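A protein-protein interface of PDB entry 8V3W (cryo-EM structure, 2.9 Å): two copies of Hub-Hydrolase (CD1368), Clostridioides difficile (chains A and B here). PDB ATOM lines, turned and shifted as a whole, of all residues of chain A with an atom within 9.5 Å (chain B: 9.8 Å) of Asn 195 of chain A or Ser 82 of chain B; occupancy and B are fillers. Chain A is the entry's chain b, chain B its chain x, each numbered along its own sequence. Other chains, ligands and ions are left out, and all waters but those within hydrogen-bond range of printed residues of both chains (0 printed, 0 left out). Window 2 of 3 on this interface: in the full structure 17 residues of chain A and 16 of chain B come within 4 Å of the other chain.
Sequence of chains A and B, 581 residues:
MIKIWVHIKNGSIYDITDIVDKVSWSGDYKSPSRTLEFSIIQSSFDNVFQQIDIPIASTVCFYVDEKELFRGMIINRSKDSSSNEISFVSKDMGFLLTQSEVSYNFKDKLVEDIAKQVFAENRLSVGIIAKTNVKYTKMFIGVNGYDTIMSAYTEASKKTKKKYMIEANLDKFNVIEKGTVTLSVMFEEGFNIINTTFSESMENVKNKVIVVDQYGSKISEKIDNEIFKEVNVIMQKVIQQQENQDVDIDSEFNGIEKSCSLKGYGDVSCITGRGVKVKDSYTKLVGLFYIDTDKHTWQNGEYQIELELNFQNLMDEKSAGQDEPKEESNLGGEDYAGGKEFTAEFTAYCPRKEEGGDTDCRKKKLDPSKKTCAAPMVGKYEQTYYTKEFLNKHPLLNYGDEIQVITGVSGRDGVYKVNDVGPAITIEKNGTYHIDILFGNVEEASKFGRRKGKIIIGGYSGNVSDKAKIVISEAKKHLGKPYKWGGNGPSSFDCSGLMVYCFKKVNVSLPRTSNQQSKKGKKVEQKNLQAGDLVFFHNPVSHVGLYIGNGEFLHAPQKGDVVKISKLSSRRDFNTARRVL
No position is printed for both chains.
Of chain B, only Asp 80, Ser 81 and Ser 82 come within 4 Å of Asn 195 of chain A. Printed residues of chain A within 4 Å of Ser 82 of chain B: Asn 195 (3.3 Å). No residue of chain B comes within 4 Å of Ile 194 of chain A. No residue of chain B comes within 4 Å of Leu 262 of chain A. Printed residues of chain A within 4 Å of Ser 81 of chain B: Asn 195 and Thr 196. No residue of chain A comes within 4 Å of Ser 83 of chain B. Of the printed residues of chain B, Thr 197 of chain A touches Lys 79 (3.4 Å) and Asp 80 (3.7 Å). Of the printed residues of chain A, Asp 80 of chain B touches Asn 195 (3.4 Å), Thr 196 (3.4 Å) and Thr 197 (3.7 Å). Ser 44 of chain B touches none of the printed residues of chain A. The nearest residue of chain A that does not touch Ser 82 of chain B is Thr 196 of chain A (5.0 Å). The nearest printed residue of chain B that does not touch Phe 198 of chain A is Ser 81 of chain B (4.5 Å).
Ser 81 of chain B touches Asn 195 of chain A. Thr 197 of chain A touches Lys 79 of chain B (CA to O, 3.4 Å). Thr 197 of chain A touches Asp 80 of chain B (OG1 to OD1, 3.7 Å).
ND2 of Asn 195 of chain A sits at hydrogen-bond distance from OD1 of Asp 80 of chain B (3.4 Å). The side-chain hydroxyl (OG1) of Thr 196 of chain A lies within hydrogen-bond range of the side-chain hydroxyl (OG) of Ser 81 of chain B, 3.0 Å away. The side-chain carboxylate (OD1) of Asp 80 of chain B lies close to the backbone carbonyl oxygen (O) of Thr 196 of chain A, at 3.4 Å. The backbone NH (N) of Ser 82 of chain B is in hydrogen-bond range of the side-chain amide oxygen (OD1) of Asn 195 of chain A (3.3 Å). The backbone NH (N) of Lys 79 of chain B is in hydrogen-bond range of the backbone carbonyl oxygen (O) of Phe 198 of chain A (2.9 Å).
Printed residues of chain B that touch a printed residue of chain A: Lys 79, Asp 80, Ser 81 and Ser 82. Of the 22 printed residues of chain A, 4 touch a printed residue of chain B. Printed residues of chain A that touch a printed residue of chain B: Asn 195, Thr 196, Thr 197 and Phe 198. Among the printed residues, no Asp or Glu carboxylate lies within 4 Å of a Lys or Arg side-chain nitrogen of the other chain.
O of Gln 42 of chain B lies within hydrogen-bond range of NZ of Lys 79 of chain B. The side-chain amino group of Lys 79 of chain B lies within hydrogen-bond range of the backbone carbonyl oxygen of Ser 83 of chain B (3.3 Å). The side-chain carboxylate (OD1) of Asp 80 of chain B is in hydrogen-bond range of the backbone NH (N) of Ser 82 of chain B (3.3 Å). O of Asn 195 of chain A is in hydrogen-bond range of N of Lys 263 of chain A, 3.1 Å away. O of Thr 197 of chain A sits at hydrogen-bond distance from N of Ser 261 of chain A.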
ATOM      1  N   PHE A 187       4.721   0.712   8.767  1.00  0.00           N
ATOM      2  CA  PHE A 187       5.853   0.236   7.986  1.00  0.00           C
ATOM      3  C   PHE A 187       5.357  -0.301   6.649  1.00  0.00           C
ATOM      4  O   PHE A 187       4.484  -1.173   6.611  1.00  0.00           O
ATOM      5  CB  PHE A 187       6.620  -0.835   8.759  1.00  0.00           C
ATOM      6  CG  PHE A 187       7.438  -0.286   9.889  1.00  0.00           C
ATOM      7  CD1 PHE A 187       8.678   0.269   9.652  1.00  0.00           C
ATOM      8  CD2 PHE A 187       6.961  -0.313  11.185  1.00  0.00           C
ATOM      9  CE1 PHE A 187       9.426   0.782  10.682  1.00  0.00           C
ATOM     10  CE2 PHE A 187       7.706   0.199  12.217  1.00  0.00           C
ATOM     11  CZ  PHE A 187       8.940   0.747  11.966  1.00  0.00           C
ATOM     12  N   GLU A 188       5.905   0.228   5.558  1.00  0.00           N
ATOM     13  CA  GLU A 188       5.575  -0.210   4.212  1.00  0.00           C
ATOM     14  C   GLU A 188       6.851  -0.569   3.470  1.00  0.00           C
ATOM     15  O   GLU A 188       7.918  -0.010   3.734  1.00  0.00           O
ATOM     16  CB  GLU A 188       4.824   0.863   3.423  1.00  0.00           C
ATOM     17  CG  GLU A 188       3.791   1.621   4.219  1.00  0.00           C
ATOM     18  CD  GLU A 188       2.685   2.182   3.348  1.00  0.00           C
ATOM     19  OE1 GLU A 188       2.937   2.437   2.154  1.00  0.00           O
ATOM     20  OE2 GLU A 188       1.566   2.373   3.862  1.00  0.00           O
ATOM     21  N   GLU A 189       6.725  -1.504   2.530  1.00  0.00           N
ATOM     22  CA  GLU A 189       7.897  -2.019   1.831  1.00  0.00           C
ATOM     23  C   GLU A 189       8.586  -0.933   1.017  1.00  0.00           C
ATOM     24  O   GLU A 189       9.817  -0.836   1.021  1.00  0.00           O
ATOM     25  CB  GLU A 189       7.500  -3.190   0.935  1.00  0.00           C
ATOM     26  CG  GLU A 189       8.650  -4.110   0.591  1.00  0.00           C
ATOM     27  CD  GLU A 189       8.242  -5.567   0.525  1.00  0.00           C
ATOM     28  OE1 GLU A 189       7.270  -5.946   1.207  1.00  0.00           O
ATOM     29  OE2 GLU A 189       8.897  -6.338  -0.205  1.00  0.00           O
ATOM     30  N   ASN A 192       9.932   2.687   4.203  1.00  0.00           N
ATOM     31  CA  ASN A 192      10.853   2.796   5.330  1.00  0.00           C
ATOM     32  C   ASN A 192      11.278   1.443   5.889  1.00  0.00           C
ATOM     33  O   ASN A 192      11.582   1.336   7.080  1.00  0.00           O
ATOM     34  CB  ASN A 192      10.246   3.640   6.453  1.00  0.00           C
ATOM     35  CG  ASN A 192       8.907   3.115   6.920  1.00  0.00           C
ATOM     36  OD1 ASN A 192       8.416   2.109   6.423  1.00  0.00           O
ATOM     37  ND2 ASN A 192       8.315   3.791   7.891  1.00  0.00           N
ATOM     38  N   ILE A 193      11.323   0.404   5.066  1.00  0.00           N
ATOM     39  CA  ILE A 193      11.721  -0.926   5.513  1.00  0.00           C
ATOM     40  C   ILE A 193      13.042  -1.288   4.853  1.00  0.00           C
ATOM     41  O   ILE A 193      13.173  -1.209   3.627  1.00  0.00           O
ATOM     42  CB  ILE A 193      10.644  -1.978   5.201  1.00  0.00           C
ATOM     43  CG1 ILE A 193       9.442  -1.795   6.121  1.00  0.00           C
ATOM     44  CG2 ILE A 193      11.201  -3.372   5.366  1.00  0.00           C
ATOM     45  CD1 ILE A 193       8.303  -2.728   5.816  1.00  0.00           C
ATOM     46  N   ILE A 194      14.020  -1.677   5.662  1.00  0.00           N
ATOM     47  CA  ILE A 194      15.285  -2.172   5.136  1.00  0.00           C
ATOM     48  C   ILE A 194      15.205  -3.657   4.817  1.00  0.00           C
ATOM     49  O   ILE A 194      15.580  -4.087   3.725  1.00  0.00           O
ATOM     50  CB  ILE A 194      16.429  -1.870   6.126  1.00  0.00           C
ATOM     51  CG1 ILE A 194      16.622  -0.362   6.271  1.00  0.00           C
ATOM     52  CG2 ILE A 194      17.715  -2.514   5.657  1.00  0.00           C
ATOM     53  CD1 ILE A 194      17.531   0.025   7.403  1.00  0.00           C
ATOM     54  N   ASN A 195      14.703  -4.461   5.751  1.00  0.00           N
ATOM     55  CA  ASN A 195      14.559  -5.891   5.524  1.00  0.00           C
ATOM     56  C   ASN A 195      13.549  -6.451   6.513  1.00  0.00           C
ATOM     57  O   ASN A 195      13.304  -5.868   7.569  1.00  0.00           O
ATOM     58  CB  ASN A 195      15.903  -6.613   5.655  1.00  0.00           C
ATOM     59  CG  ASN A 195      15.961  -7.886   4.839  1.00  0.00           C
ATOM     60  OD1 ASN A 195      15.342  -7.987   3.782  1.00  0.00           O
ATOM     61  ND2 ASN A 195      16.702  -8.870   5.329  1.00  0.00           N
ATOM     62  N   THR A 196      12.965  -7.594   6.154  1.00  0.00           N
ATOM     63  CA  THR A 196      12.037  -8.308   7.021  1.00  0.00           C
ATOM     64  C   THR A 196      12.240  -9.806   6.860  1.00  0.00           C
ATOM     65  O   THR A 196      12.747 -10.278   5.842  1.00  0.00           O
ATOM     66  CB  THR A 196      10.574  -7.964   6.717  1.00  0.00           C
ATOM     67  OG1 THR A 196      10.392  -7.858   5.302  1.00  0.00           O
ATOM     68  CG2 THR A 196      10.178  -6.658   7.369  1.00  0.00           C
ATOM     69  N   THR A 197      11.830 -10.555   7.881  1.00  0.00           N
ATOM     70  CA  THR A 197      11.840 -12.012   7.831  1.00  0.00           C
ATOM     71  C   THR A 197      10.613 -12.531   8.562  1.00  0.00           C
ATOM     72  O   THR A 197      10.474 -12.315   9.767  1.00  0.00           O
ATOM     73  CB  THR A 197      13.114 -12.586   8.455  1.00  0.00           C
ATOM     74  OG1 THR A 197      14.261 -12.027   7.807  1.00  0.00           O
ATOM     75  CG2 THR A 197      13.151 -14.088   8.287  1.00  0.00           C
ATOM     76  N   PHE A 198       9.731 -13.213   7.840  1.00  0.00           N
ATOM     77  CA  PHE A 198       8.505 -13.758   8.403  1.00  0.00           C
ATOM     78  C   PHE A 198       8.664 -15.248   8.660  1.00  0.00           C
ATOM     79  O   PHE A 198       9.283 -15.961   7.868  1.00  0.00           O
ATOM     80  CB  PHE A 198       7.324 -13.520   7.466  1.00  0.00           C
ATOM     81  CG  PHE A 198       7.050 -12.076   7.196  1.00  0.00           C
ATOM     82  CD1 PHE A 198       6.284 -11.329   8.067  1.00  0.00           C
ATOM     83  CD2 PHE A 198       7.555 -11.466   6.067  1.00  0.00           C
ATOM     84  CE1 PHE A 198       6.027 -10.002   7.815  1.00  0.00           C
ATOM     85  CE2 PHE A 198       7.303 -10.141   5.815  1.00  0.00           C
ATOM     86  CZ  PHE A 198       6.542  -9.409   6.691  1.00  0.00           C
ATOM     87  N   CYS A 260       7.556 -11.795  13.015  1.00  0.00           N
ATOM     88  CA  CYS A 260       8.288 -11.007  12.034  1.00  0.00           C
ATOM     89  C   CYS A 260       9.498 -10.369  12.701  1.00  0.00           C
ATOM     90  O   CYS A 260       9.445  -9.992  13.873  1.00  0.00           O
ATOM     91  CB  CYS A 260       7.402  -9.928  11.406  1.00  0.00           C
ATOM     92  SG  CYS A 260       8.248  -8.879  10.206  1.00  0.00           S
ATOM     93  N   SER A 261      10.585 -10.261  11.947  1.00  0.00           N
ATOM     94  CA  SER A 261      11.810  -9.597  12.377  1.00  0.00           C
ATOM     95  C   SER A 261      12.064  -8.450  11.411  1.00  0.00           C
ATOM     96  O   SER A 261      12.326  -8.681  10.229  1.00  0.00           O
ATOM     97  CB  SER A 261      12.979 -10.578  12.393  1.00  0.00           C
ATOM     98  OG  SER A 261      13.932 -10.232  13.377  1.00  0.00           O
ATOM     99  N   LEU A 262      11.999  -7.220  11.906  1.00  0.00           N
ATOM    100  CA  LEU A 262      11.977  -6.041  11.053  1.00  0.00           C
ATOM    101  C   LEU A 262      13.123  -5.099  11.398  1.00  0.00           C
ATOM    102  O   LEU A 262      13.443  -4.900  12.571  1.00  0.00           O
ATOM    103  CB  LEU A 262      10.638  -5.313  11.186  1.00  0.00           C
ATOM    104  CG  LEU A 262      10.328  -4.146  10.252  1.00  0.00           C
ATOM    105  CD1 LEU A 262       8.864  -4.161   9.884  1.00  0.00           C
ATOM    106  CD2 LEU A 262      10.685  -2.830  10.901  1.00  0.00           C
ATOM    107  N   LYS A 263      13.734  -4.524  10.367  1.00  0.00           N
ATOM    108  CA  LYS A 263      14.737  -3.479  10.515  1.00  0.00           C
ATOM    109  C   LYS A 263      14.391  -2.336   9.574  1.00  0.00           C
ATOM    110  O   LYS A 263      14.160  -2.564   8.384  1.00  0.00           O
ATOM    111  CB  LYS A 263      16.137  -4.015  10.217  1.00  0.00           C
ATOM    112  CG  LYS A 263      17.209  -2.960  10.175  1.00  0.00           C
ATOM    113  CD  LYS A 263      18.571  -3.578  10.399  1.00  0.00           C
ATOM    114  CE  LYS A 263      19.679  -2.650   9.950  1.00  0.00           C
ATOM    115  NZ  LYS A 263      19.976  -2.796   8.503  1.00  0.00           N
ATOM    116  N   GLY A 264      14.349  -1.118  10.097  1.00  0.00           N
ATOM    117  CA  GLY A 264      13.936   0.004   9.283  1.00  0.00           C
ATOM    118  C   GLY A 264      14.096   1.329   9.991  1.00  0.00           C
ATOM    119  O   GLY A 264      14.867   1.456  10.940  1.00  0.00           O
ATOM    120  N   TYR A 265      13.352   2.321   9.508  1.00  0.00           N
ATOM    121  CA  TYR A 265      13.407   3.684  10.021  1.00  0.00           C
ATOM    122  C   TYR A 265      12.107   4.034  10.728  1.00  0.00           C
ATOM    123  O   TYR A 265      11.021   3.777  10.204  1.00  0.00           O
ATOM    124  CB  TYR A 265      13.664   4.679   8.893  1.00  0.00           C
ATOM    125  CG  TYR A 265      15.014   4.521   8.257  1.00  0.00           C
ATOM    126  CD1 TYR A 265      16.160   4.930   8.913  1.00  0.00           C
ATOM    127  CD2 TYR A 265      15.145   3.954   7.003  1.00  0.00           C
ATOM    128  CE1 TYR A 265      17.396   4.785   8.338  1.00  0.00           C
ATOM    129  CE2 TYR A 265      16.378   3.804   6.419  1.00  0.00           C
ATOM    130  CZ  TYR A 265      17.500   4.222   7.092  1.00  0.00           C
ATOM    131  OH  TYR A 265      18.737   4.077   6.519  1.00  0.00           O
ATOM    132  N   VAL A 278       1.960  -3.172   9.886  1.00  0.00           N
ATOM    133  CA  VAL A 278       2.809  -3.503   8.748  1.00  0.00           C
ATOM    134  C   VAL A 278       1.913  -3.836   7.565  1.00  0.00           C
ATOM    135  O   VAL A 278       0.956  -4.602   7.706  1.00  0.00           O
ATOM    136  CB  VAL A 278       3.756  -4.680   9.054  1.00  0.00           C
ATOM    137  CG1 VAL A 278       4.853  -4.752   8.021  1.00  0.00           C
ATOM    138  CG2 VAL A 278       4.346  -4.545  10.445  1.00  0.00           C
ATOM    139  N   GLN A 304      18.785   3.761  13.187  1.00  0.00           N
ATOM    140  CA  GLN A 304      18.027   2.613  12.705  1.00  0.00           C
ATOM    141  C   GLN A 304      17.408   1.872  13.882  1.00  0.00           C
ATOM    142  O   GLN A 304      17.874   1.975  15.016  1.00  0.00           O
ATOM    143  CB  GLN A 304      18.909   1.660  11.894  1.00  0.00           C
ATOM    144  CG  GLN A 304      19.332   2.203  10.546  1.00  0.00           C
ATOM    145  CD  GLN A 304      20.442   1.393   9.919  1.00  0.00           C
ATOM    146  OE1 GLN A 304      20.805   0.335  10.418  1.00  0.00           O
ATOM    147  NE2 GLN A 304      20.984   1.887   8.817  1.00  0.00           N
ATOM    148  N   ILE A 305      16.346   1.115  13.597  1.00  0.00           N
ATOM    149  CA  ILE A 305      15.610   0.365  14.608  1.00  0.00           C
ATOM    150  C   ILE A 305      15.524  -1.099  14.196  1.00  0.00           C
ATOM    151  O   ILE A 305      15.520  -1.426  13.007  1.00  0.00           O
ATOM    152  CB  ILE A 305      14.194   0.938  14.828  1.00  0.00           C
ATOM    153  CG1 ILE A 305      14.238   2.458  14.882  1.00  0.00           C
ATOM    154  CG2 ILE A 305      13.591   0.416  16.110  1.00  0.00           C
ATOM    155  CD1 ILE A 305      12.890   3.076  15.082  1.00  0.00           C
ATOM    156  N   GLU A 306      15.450  -1.982  15.192  1.00  0.00           N
ATOM    157  CA  GLU A 306      15.230  -3.409  14.981  1.00  0.00           C
ATOM    158  C   GLU A 306      14.150  -3.893  15.935  1.00  0.00           C
ATOM    159  O   GLU A 306      14.282  -3.733  17.149  1.00  0.00           O
ATOM    160  CB  GLU A 306      16.515  -4.209  15.200  1.00  0.00           C
ATOM    161  CG  GLU A 306      17.534  -4.056  14.101  1.00  0.00           C
ATOM    162  CD  GLU A 306      18.843  -4.745  14.421  1.00  0.00           C
ATOM    163  OE1 GLU A 306      19.069  -5.078  15.602  1.00  0.00           O
ATOM    164  OE2 GLU A 306      19.649  -4.956  13.492  1.00  0.00           O
ATOM    165  N   LEU A 307      13.099  -4.502  15.393  1.00  0.00           N
ATOM    166  CA  LEU A 307      11.943  -4.901  16.183  1.00  0.00           C
ATOM    167  C   LEU A 307      11.664  -6.386  16.020  1.00  0.00           C
ATOM    168  O   LEU A 307      11.896  -6.968  14.960  1.00  0.00           O
ATOM    169  CB  LEU A 307      10.691  -4.119  15.784  1.00  0.00           C
ATOM    170  CG  LEU A 307      10.819  -2.605  15.666  1.00  0.00           C
ATOM    171  CD1 LEU A 307       9.644  -2.048  14.896  1.00  0.00           C
ATOM    172  CD2 LEU A 307      10.910  -1.971  17.034  1.00  0.00           C
ATOM    173  N   LEU A 309       8.385  -8.694  16.267  1.00  0.00           N
ATOM    174  CA  LEU A 309       6.950  -8.467  16.224  1.00  0.00           C
ATOM    175  C   LEU A 309       6.192  -9.782  16.325  1.00  0.00           C
ATOM    176  O   LEU A 309       6.630 -10.813  15.812  1.00  0.00           O
ATOM    177  CB  LEU A 309       6.559  -7.739  14.939  1.00  0.00           C
ATOM    178  CG  LEU A 309       7.329  -6.446  14.679  1.00  0.00           C
ATOM    179  CD1 LEU A 309       7.073  -5.938  13.282  1.00  0.00           C
ATOM    180  CD2 LEU A 309       6.959  -5.393  15.701  1.00  0.00           C
ATOM    181  N   GLN B  42      11.012 -18.657  -4.427  1.00  0.00           N
ATOM    182  CA  GLN B  42       9.761 -17.931  -4.563  1.00  0.00           C
ATOM    183  C   GLN B  42      10.099 -16.461  -4.427  1.00  0.00           C
ATOM    184  O   GLN B  42      10.669 -16.047  -3.412  1.00  0.00           O
ATOM    185  CB  GLN B  42       8.757 -18.356  -3.494  1.00  0.00           C
ATOM    186  CG  GLN B  42       7.324 -18.018  -3.827  1.00  0.00           C
ATOM    187  CD  GLN B  42       6.937 -16.617  -3.392  1.00  0.00           C
ATOM    188  OE1 GLN B  42       7.675 -15.950  -2.666  1.00  0.00           O
ATOM    189  NE2 GLN B  42       5.774 -16.165  -3.838  1.00  0.00           N
ATOM    190  N   SER B  43       9.763 -15.678  -5.441  1.00  0.00           N
ATOM    191  CA  SER B  43      10.067 -14.259  -5.452  1.00  0.00           C
ATOM    192  C   SER B  43       8.773 -13.461  -5.420  1.00  0.00           C
ATOM    193  O   SER B  43       7.847 -13.722  -6.193  1.00  0.00           O
ATOM    194  CB  SER B  43      10.892 -13.881  -6.685  1.00  0.00           C
ATOM    195  OG  SER B  43      11.194 -12.500  -6.696  1.00  0.00           O
ATOM    196  N   SER B  44       8.717 -12.492  -4.513  1.00  0.00           N
ATOM    197  CA  SER B  44       7.569 -11.604  -4.409  1.00  0.00           C
ATOM    198  C   SER B  44       7.717 -10.368  -5.283  1.00  0.00           C
ATOM    199  O   SER B  44       6.711  -9.791  -5.709  1.00  0.00           O
ATOM    200  CB  SER B  44       7.366 -11.190  -2.951  1.00  0.00           C
ATOM    201  OG  SER B  44       8.607 -10.869  -2.345  1.00  0.00           O
ATOM    202  N   PHE B  45       8.956  -9.952  -5.550  1.00  0.00           N
ATOM    203  CA  PHE B  45       9.191  -8.825  -6.442  1.00  0.00           C
ATOM    204  C   PHE B  45       8.776  -9.154  -7.871  1.00  0.00           C
ATOM    205  O   PHE B  45       8.129  -8.340  -8.540  1.00  0.00           O
ATOM    206  CB  PHE B  45      10.667  -8.425  -6.378  1.00  0.00           C
ATOM    207  CG  PHE B  45      10.933  -6.982  -6.712  1.00  0.00           C
ATOM    208  CD1 PHE B  45       9.937  -6.174  -7.234  1.00  0.00           C
ATOM    209  CD2 PHE B  45      12.188  -6.434  -6.503  1.00  0.00           C
ATOM    210  CE1 PHE B  45      10.190  -4.852  -7.544  1.00  0.00           C
ATOM    211  CE2 PHE B  45      12.444  -5.112  -6.809  1.00  0.00           C
ATOM    212  CZ  PHE B  45      11.443  -4.322  -7.331  1.00  0.00           C
ATOM    213  N   LYS B  79      10.581 -17.040   5.561  1.00  0.00           N
ATOM    214  CA  LYS B  79      10.694 -16.297   4.311  1.00  0.00           C
ATOM    215  C   LYS B  79      11.510 -15.036   4.546  1.00  0.00           C
ATOM    216  O   LYS B  79      11.164 -14.222   5.405  1.00  0.00           O
ATOM    217  CB  LYS B  79       9.314 -15.943   3.755  1.00  0.00           C
ATOM    218  CG  LYS B  79       9.325 -14.888   2.673  1.00  0.00           C
ATOM    219  CD  LYS B  79      10.061 -15.372   1.444  1.00  0.00           C
ATOM    220  CE  LYS B  79      10.025 -14.339   0.337  1.00  0.00           C
ATOM    221  NZ  LYS B  79      10.994 -14.661  -0.748  1.00  0.00           N
ATOM    222  N   ASP B  80      12.578 -14.876   3.776  1.00  0.00           N
ATOM    223  CA  ASP B  80      13.446 -13.707   3.839  1.00  0.00           C
ATOM    224  C   ASP B  80      13.144 -12.806   2.649  1.00  0.00           C
ATOM    225  O   ASP B  80      13.045 -13.283   1.516  1.00  0.00           O
ATOM    226  CB  ASP B  80      14.912 -14.137   3.833  1.00  0.00           C
ATOM    227  CG  ASP B  80      15.859 -12.995   4.120  1.00  0.00           C
ATOM    228  OD1 ASP B  80      15.395 -11.851   4.288  1.00  0.00           O
ATOM    229  OD2 ASP B  80      17.079 -13.245   4.179  1.00  0.00           O
ATOM    230  N   SER B  81      12.979 -11.509   2.908  1.00  0.00           N
ATOM    231  CA  SER B  81      12.561 -10.601   1.844  1.00  0.00           C
ATOM    232  C   SER B  81      13.701 -10.265   0.893  1.00  0.00           C
ATOM    233  O   SER B  81      13.455  -9.969  -0.281  1.00  0.00           O
ATOM    234  CB  SER B  81      11.976  -9.323   2.436  1.00  0.00           C
ATOM    235  OG  SER B  81      10.646  -9.535   2.874  1.00  0.00           O
ATOM    236  N   SER B  82      14.942 -10.275   1.376  1.00  0.00           N
ATOM    237  CA  SER B  82      16.071  -9.984   0.500  1.00  0.00           C
ATOM    238  C   SER B  82      16.297 -11.115  -0.495  1.00  0.00           C
ATOM    239  O   SER B  82      16.438 -10.876  -1.700  1.00  0.00           O
ATOM    240  CB  SER B  82      17.328  -9.739   1.331  1.00  0.00           C
ATOM    241  OG  SER B  82      17.852 -10.955   1.835  1.00  0.00           O
ATOM    242  N   SER B  83      16.321 -12.352  -0.012  1.00  0.00           N
ATOM    243  CA  SER B  83      16.604 -13.509  -0.847  1.00  0.00           C
ATOM    244  C   SER B  83      15.312 -14.103  -1.384  1.00  0.00           C
ATOM    245  O   SER B  83      14.288 -14.115  -0.699  1.00  0.00           O
ATOM    246  CB  SER B  83      17.368 -14.567  -0.055  1.00  0.00           C
ATOM    247  OG  SER B  83      17.588 -15.724  -0.840  1.00  0.00           O
ATOM    248  N   ASN B  84      15.364 -14.595  -2.619  1.00  0.00           N
ATOM    249  CA  ASN B  84      14.191 -15.199  -3.249  1.00  0.00           C
ATOM    250  C   ASN B  84      14.129 -16.689  -2.910  1.00  0.00           C
ATOM    251  O   ASN B  84      14.292 -17.563  -3.760  1.00  0.00           O
ATOM    252  CB  ASN B  84      14.224 -14.964  -4.754  1.00  0.00           C
ATOM    253  CG  ASN B  84      15.618 -15.086  -5.331  1.00  0.00           C
ATOM    254  OD1 ASN B  84      16.387 -15.960  -4.941  1.00  0.00           O
ATOM    255  ND2 ASN B  84      15.951 -14.207  -6.267  1.00  0.00           N
ATOM    256  N   GLU B  85      13.863 -16.968  -1.633  1.00  0.00           N
ATOM    257  CA  GLU B  85      13.881 -18.336  -1.129  1.00  0.00           C
ATOM    258  C   GLU B  85      12.918 -18.471   0.042  1.00  0.00           C
ATOM    259  O   GLU B  85      12.706 -17.524   0.800  1.00  0.00           O
ATOM    260  CB  GLU B  85      15.283 -18.747  -0.671  1.00  0.00           C
ATOM    261  CG  GLU B  85      16.309 -18.878  -1.768  1.00  0.00           C
ATOM    262  CD  GLU B  85      17.382 -19.879  -1.432  1.00  0.00           C
ATOM    263  OE1 GLU B  85      17.507 -20.240  -0.244  1.00  0.00           O
ATOM    264  OE2 GLU B  85      18.112 -20.292  -2.351  1.00  0.00           O
ATOM    265  N   ILE B  86      12.358 -19.670   0.186  1.00  0.00           N
ATOM    266  CA  ILE B  86      11.545 -20.053   1.335  1.00  0.00           C
ATOM    267  C   ILE B  86      12.124 -21.339   1.906  1.00  0.00           C
ATOM    268  O   ILE B  86      12.437 -22.265   1.151  1.00  0.00           O
ATOM    269  CB  ILE B  86      10.064 -20.249   0.958  1.00  0.00           C
ATOM    270  CG1 ILE B  86       9.525 -19.023   0.227  1.00  0.00           C
ATOM    271  CG2 ILE B  86       9.228 -20.527   2.187  1.00  0.00           C
ATOM    272  CD1 ILE B  86       8.039 -19.056   0.020  1.00  0.00           C
